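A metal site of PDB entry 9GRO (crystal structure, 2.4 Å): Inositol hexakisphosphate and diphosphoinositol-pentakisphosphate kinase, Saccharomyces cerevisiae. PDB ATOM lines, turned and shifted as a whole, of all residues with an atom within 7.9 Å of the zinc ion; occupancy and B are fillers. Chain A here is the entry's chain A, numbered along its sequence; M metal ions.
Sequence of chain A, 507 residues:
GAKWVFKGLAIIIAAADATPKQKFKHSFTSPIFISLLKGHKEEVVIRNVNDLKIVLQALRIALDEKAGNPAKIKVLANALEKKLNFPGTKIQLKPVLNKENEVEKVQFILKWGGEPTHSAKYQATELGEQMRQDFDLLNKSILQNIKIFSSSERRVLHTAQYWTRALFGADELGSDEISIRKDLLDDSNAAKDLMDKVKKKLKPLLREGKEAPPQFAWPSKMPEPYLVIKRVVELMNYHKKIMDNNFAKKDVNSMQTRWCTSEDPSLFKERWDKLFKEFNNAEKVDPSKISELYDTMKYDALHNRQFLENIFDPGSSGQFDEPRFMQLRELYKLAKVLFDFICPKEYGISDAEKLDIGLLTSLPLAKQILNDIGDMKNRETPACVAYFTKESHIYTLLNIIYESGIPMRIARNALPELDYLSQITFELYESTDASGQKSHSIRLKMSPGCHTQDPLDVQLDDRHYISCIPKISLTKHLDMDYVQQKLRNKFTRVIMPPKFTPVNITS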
ATOM      1  N   ASP A  17       2.066  27.897 -31.374  1.00  0.00           N
ATOM      2  CA  ASP A  17       1.745  27.076 -30.210  1.00  0.00           C
ATOM      3  C   ASP A  17       1.326  25.675 -30.626  1.00  0.00           C
ATOM      4  O   ASP A  17       0.548  25.490 -31.561  1.00  0.00           O
ATOM      5  CB  ASP A  17       0.622  27.749 -29.408  1.00  0.00           C
ATOM      6  CG  ASP A  17       0.390  27.102 -28.059  1.00  0.00           C
ATOM      7  OD1 ASP A  17       1.343  27.024 -27.265  1.00  0.00           O
ATOM      8  OD2 ASP A  17      -0.755  26.682 -27.790  1.00  0.00           O
ATOM      9  N   THR A 117      -2.033  23.777 -31.674  1.00  0.00           N
ATOM     10  CA  THR A 117      -3.203  23.998 -30.847  1.00  0.00           C
ATOM     11  C   THR A 117      -4.169  24.941 -31.562  1.00  0.00           C
ATOM     12  O   THR A 117      -3.870  25.526 -32.606  1.00  0.00           O
ATOM     13  CB  THR A 117      -2.809  24.578 -29.495  1.00  0.00           C
ATOM     14  OG1 THR A 117      -2.327  25.924 -29.668  1.00  0.00           O
ATOM     15  CG2 THR A 117      -1.726  23.730 -28.836  1.00  0.00           C
ATOM     16  N   HIS A 118      -5.371  25.075 -30.981  1.00  0.00           N
ATOM     17  CA  HIS A 118      -6.324  26.039 -31.507  1.00  0.00           C
ATOM     18  C   HIS A 118      -5.792  27.470 -31.402  1.00  0.00           C
ATOM     19  O   HIS A 118      -6.272  28.350 -32.115  1.00  0.00           O
ATOM     20  CB  HIS A 118      -7.651  25.928 -30.753  1.00  0.00           C
ATOM     21  CG  HIS A 118      -7.576  26.377 -29.327  1.00  0.00           C
ATOM     22  ND1 HIS A 118      -8.061  27.598 -28.911  1.00  0.00           N
ATOM     23  CD2 HIS A 118      -7.060  25.785 -28.226  1.00  0.00           C
ATOM     24  CE1 HIS A 118      -7.862  27.729 -27.612  1.00  0.00           C
ATOM     25  NE2 HIS A 118      -7.247  26.644 -27.175  1.00  0.00           N
ATOM     26  N   SER A 119      -4.796  27.700 -30.539  1.00  0.00           N
ATOM     27  CA  SER A 119      -4.240  29.040 -30.364  1.00  0.00           C
ATOM     28  C   SER A 119      -3.216  29.407 -31.439  1.00  0.00           C
ATOM     29  O   SER A 119      -2.938  30.587 -31.625  1.00  0.00           O
ATOM     30  CB  SER A 119      -3.583  29.158 -28.986  1.00  0.00           C
ATOM     31  OG  SER A 119      -4.507  28.871 -27.956  1.00  0.00           O
ATOM     32  N   CYS A 260     -12.110  21.028 -23.270  1.00  0.00           N
ATOM     33  CA  CYS A 260     -12.117  21.088 -24.722  1.00  0.00           C
ATOM     34  C   CYS A 260     -11.244  19.961 -25.275  1.00  0.00           C
ATOM     35  O   CYS A 260     -10.522  19.284 -24.533  1.00  0.00           O
ATOM     36  CB  CYS A 260     -11.612  22.434 -25.259  1.00  0.00           C
ATOM     37  SG  CYS A 260     -12.559  23.890 -24.740  1.00  0.00           S
ATOM     38  N   THR A 261     -11.320  19.770 -26.584  1.00  0.00           N
ATOM     39  CA  THR A 261     -10.434  18.832 -27.273  1.00  0.00           C
ATOM     40  C   THR A 261      -8.989  19.098 -26.865  1.00  0.00           C
ATOM     41  O   THR A 261      -8.506  20.238 -26.962  1.00  0.00           O
ATOM     42  CB  THR A 261     -10.604  18.979 -28.780  1.00  0.00           C
ATOM     43  OG1 THR A 261     -11.977  18.745 -29.138  1.00  0.00           O
ATOM     44  CG2 THR A 261      -9.711  17.988 -29.526  1.00  0.00           C
ATOM     45  N   SER A 262      -8.299  18.054 -26.418  1.00  0.00           N
ATOM     46  CA  SER A 262      -6.916  18.096 -25.959  1.00  0.00           C
ATOM     47  C   SER A 262      -6.769  18.780 -24.602  1.00  0.00           C
ATOM     48  O   SER A 262      -5.635  19.010 -24.158  1.00  0.00           O
ATOM     49  CB  SER A 262      -6.015  18.805 -26.973  1.00  0.00           C
ATOM     50  OG  SER A 262      -6.212  18.296 -28.273  1.00  0.00           O
ATOM     51  N   GLU A 263      -7.864  19.108 -23.930  1.00  0.00           N
ATOM     52  CA  GLU A 263      -7.853  19.868 -22.689  1.00  0.00           C
ATOM     53  C   GLU A 263      -8.793  19.240 -21.660  1.00  0.00           C
ATOM     54  O   GLU A 263      -9.641  19.911 -21.066  1.00  0.00           O
ATOM     55  CB  GLU A 263      -8.232  21.327 -22.953  1.00  0.00           C
ATOM     56  CG  GLU A 263      -7.238  22.053 -23.828  1.00  0.00           C
ATOM     57  CD  GLU A 263      -7.683  23.463 -24.165  1.00  0.00           C
ATOM     58  OE1 GLU A 263      -8.762  23.887 -23.696  1.00  0.00           O
ATOM     59  OE2 GLU A 263      -6.945  24.161 -24.903  1.00  0.00           O
ATOM     60  N   TYR A 299       2.181  24.146 -21.519  1.00  0.00           N
ATOM     61  CA  TYR A 299       0.894  23.809 -22.132  1.00  0.00           C
ATOM     62  C   TYR A 299      -0.242  23.895 -21.115  1.00  0.00           C
ATOM     63  O   TYR A 299      -1.280  24.508 -21.370  1.00  0.00           O
ATOM     64  CB  TYR A 299       0.967  22.411 -22.748  1.00  0.00           C
ATOM     65  CG  TYR A 299      -0.310  21.953 -23.410  1.00  0.00           C
ATOM     66  CD1 TYR A 299      -0.642  22.391 -24.687  1.00  0.00           C
ATOM     67  CD2 TYR A 299      -1.180  21.097 -22.755  1.00  0.00           C
ATOM     68  CE1 TYR A 299      -1.812  21.975 -25.291  1.00  0.00           C
ATOM     69  CE2 TYR A 299      -2.355  20.675 -23.365  1.00  0.00           C
ATOM     70  CZ  TYR A 299      -2.665  21.117 -24.633  1.00  0.00           C
ATOM     71  OH  TYR A 299      -3.829  20.705 -25.230  1.00  0.00           O
ATOM     72  N   LEU A 302      -1.174  27.167 -19.810  1.00  0.00           N
ATOM     73  CA  LEU A 302      -1.717  27.927 -20.933  1.00  0.00           C
ATOM     74  C   LEU A 302      -3.089  27.441 -21.364  1.00  0.00           C
ATOM     75  O   LEU A 302      -3.938  28.253 -21.745  1.00  0.00           O
ATOM     76  CB  LEU A 302      -0.741  27.864 -22.111  1.00  0.00           C
ATOM     77  CG  LEU A 302      -1.047  28.622 -23.393  1.00  0.00           C
ATOM     78  CD1 LEU A 302      -1.238  30.101 -23.117  1.00  0.00           C
ATOM     79  CD2 LEU A 302       0.081  28.408 -24.391  1.00  0.00           C
ATOM     80  N   HIS A 303      -3.341  26.128 -21.311  1.00  0.00           N
ATOM     81  CA  HIS A 303      -4.563  25.552 -21.830  1.00  0.00           C
ATOM     82  C   HIS A 303      -5.413  24.819 -20.794  1.00  0.00           C
ATOM     83  O   HIS A 303      -6.595  24.574 -21.059  1.00  0.00           O
ATOM     84  CB  HIS A 303      -4.250  24.569 -22.968  1.00  0.00           C
ATOM     85  CG  HIS A 303      -3.519  25.195 -24.125  1.00  0.00           C
ATOM     86  ND1 HIS A 303      -4.167  25.907 -25.116  1.00  0.00           N
ATOM     87  CD2 HIS A 303      -2.201  25.236 -24.436  1.00  0.00           C
ATOM     88  CE1 HIS A 303      -3.284  26.343 -25.983  1.00  0.00           C
ATOM     89  NE2 HIS A 303      -2.078  25.947 -25.601  1.00  0.00           N
ATOM     90  N   ASN A 304      -4.855  24.471 -19.634  1.00  0.00           N
ATOM     91  CA  ASN A 304      -5.580  23.795 -18.549  1.00  0.00           C
ATOM     92  C   ASN A 304      -5.263  24.482 -17.219  1.00  0.00           C
ATOM     93  O   ASN A 304      -4.906  23.851 -16.228  1.00  0.00           O
ATOM     94  CB  ASN A 304      -5.217  22.314 -18.505  1.00  0.00           C
ATOM     95  CG  ASN A 304      -5.780  21.547 -19.694  1.00  0.00           C
ATOM     96  OD1 ASN A 304      -6.953  21.700 -20.045  1.00  0.00           O
ATOM     97  ND2 ASN A 304      -4.941  20.730 -20.317  1.00  0.00           N
ATOM     98  N   ASP A 461      -8.201  34.413 -21.726  1.00  0.00           N
ATOM     99  CA  ASP A 461      -9.578  34.075 -22.072  1.00  0.00           C
ATOM    100  C   ASP A 461      -9.584  32.747 -22.832  1.00  0.00           C
ATOM    101  O   ASP A 461      -8.566  32.048 -22.896  1.00  0.00           O
ATOM    102  CB  ASP A 461     -10.204  35.215 -22.873  1.00  0.00           C
ATOM    103  CG  ASP A 461      -9.438  35.529 -24.147  1.00  0.00           C
ATOM    104  OD1 ASP A 461      -8.822  34.608 -24.723  1.00  0.00           O
ATOM    105  OD2 ASP A 461      -9.442  36.703 -24.566  1.00  0.00           O
ATOM    106  N   ASP A 462     -10.723  32.398 -23.424  1.00  0.00           N
ATOM    107  CA  ASP A 462     -10.850  31.087 -24.077  1.00  0.00           C
ATOM    108  C   ASP A 462      -9.824  30.895 -25.191  1.00  0.00           C
ATOM    109  O   ASP A 462      -9.580  29.751 -25.586  1.00  0.00           O
ATOM    110  CB  ASP A 462     -12.260  30.914 -24.624  1.00  0.00           C
ATOM    111  CG  ASP A 462     -13.295  30.749 -23.534  1.00  0.00           C
ATOM    112  OD1 ASP A 462     -13.012  30.026 -22.558  1.00  0.00           O
ATOM    113  OD2 ASP A 462     -14.375  31.366 -23.630  1.00  0.00           O
ATOM    114  N   ARG A 463      -9.255  31.978 -25.724  1.00  0.00           N
ATOM    115  CA  ARG A 463      -8.273  31.831 -26.791  1.00  0.00           C
ATOM    116  C   ARG A 463      -6.975  31.190 -26.302  1.00  0.00           C
ATOM    117  O   ARG A 463      -6.285  30.534 -27.085  1.00  0.00           O
ATOM    118  CB  ARG A 463      -7.981  33.203 -27.413  1.00  0.00           C
ATOM    119  CG  ARG A 463      -9.168  33.820 -28.136  1.00  0.00           C
ATOM    120  CD  ARG A 463      -8.825  35.190 -28.677  1.00  0.00           C
ATOM    121  NE  ARG A 463      -8.606  36.156 -27.600  1.00  0.00           N
ATOM    122  CZ  ARG A 463      -8.145  37.381 -27.780  1.00  0.00           C
ATOM    123  NH1 ARG A 463      -7.814  37.839 -28.980  1.00  0.00           N
ATOM    124  NH2 ARG A 463      -7.998  38.184 -26.725  1.00  0.00           N
ATOM    125  N   HIS A 464      -6.636  31.370 -25.027  1.00  0.00           N
ATOM    126  CA  HIS A 464      -5.416  30.801 -24.466  1.00  0.00           C
ATOM    127  C   HIS A 464      -4.201  31.217 -25.296  1.00  0.00           C
ATOM    128  O   HIS A 464      -3.339  30.410 -25.649  1.00  0.00           O
ATOM    129  CB  HIS A 464      -5.508  29.275 -24.376  1.00  0.00           C
ATOM    130  CG  HIS A 464      -6.618  28.791 -23.490  1.00  0.00           C
ATOM    131  ND1 HIS A 464      -7.065  27.484 -23.506  1.00  0.00           N
ATOM    132  CD2 HIS A 464      -7.373  29.445 -22.572  1.00  0.00           C
ATOM    133  CE1 HIS A 464      -8.048  27.355 -22.633  1.00  0.00           C
ATOM    134  NE2 HIS A 464      -8.254  28.519 -22.052  1.00  0.00           N
ATOM    135  N   TYR A 465      -4.146  32.507 -25.611  1.00  0.00           N
ATOM    136  CA  TYR A 465      -3.286  33.038 -26.662  1.00  0.00           C
ATOM    137  C   TYR A 465      -2.296  34.036 -26.069  1.00  0.00           C
ATOM    138  O   TYR A 465      -2.700  34.986 -25.388  1.00  0.00           O
ATOM    139  CB  TYR A 465      -4.159  33.670 -27.750  1.00  0.00           C
ATOM    140  CG  TYR A 465      -3.518  34.756 -28.583  1.00  0.00           C
ATOM    141  CD1 TYR A 465      -2.289  34.563 -29.202  1.00  0.00           C
ATOM    142  CD2 TYR A 465      -4.170  35.974 -28.783  1.00  0.00           C
ATOM    143  CE1 TYR A 465      -1.719  35.555 -29.973  1.00  0.00           C
ATOM    144  CE2 TYR A 465      -3.607  36.965 -29.548  1.00  0.00           C
ATOM    145  CZ  TYR A 465      -2.378  36.758 -30.140  1.00  0.00           C
ATOM    146  OH  TYR A 465      -1.824  37.753 -30.915  1.00  0.00           O
HETATM  147 ZN    ZN M   1      -6.455  25.990 -25.122  1.00  0.00          ZN
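O of Glu 263 lies close to OD1 of Asn 304 (3.4 Å).
OG of Ser 119 sits at hydrogen-bond distance from O of His 464 (3.0 Å).
NE2 of His 303 is in hydrogen-bond range of OD2 of Asp 17 (2.7 Å).
Of the 17 residues printed, 4 come within 4 Å of the zinc ion.
The zinc ion is bound by the side-chain carboxylate (OE2) of Glu 263 (1.9 Å).
The zinc ion is bound by a ring nitrogen (ND1) of His 464 (2.3 Å).
ND1 of His 303 is bound to the zinc ion, 2.3 Å away.
The zinc ion is bound by NE2 of His 118 (2.3 Å).
The zinc ion has four donor atoms within binding distance.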
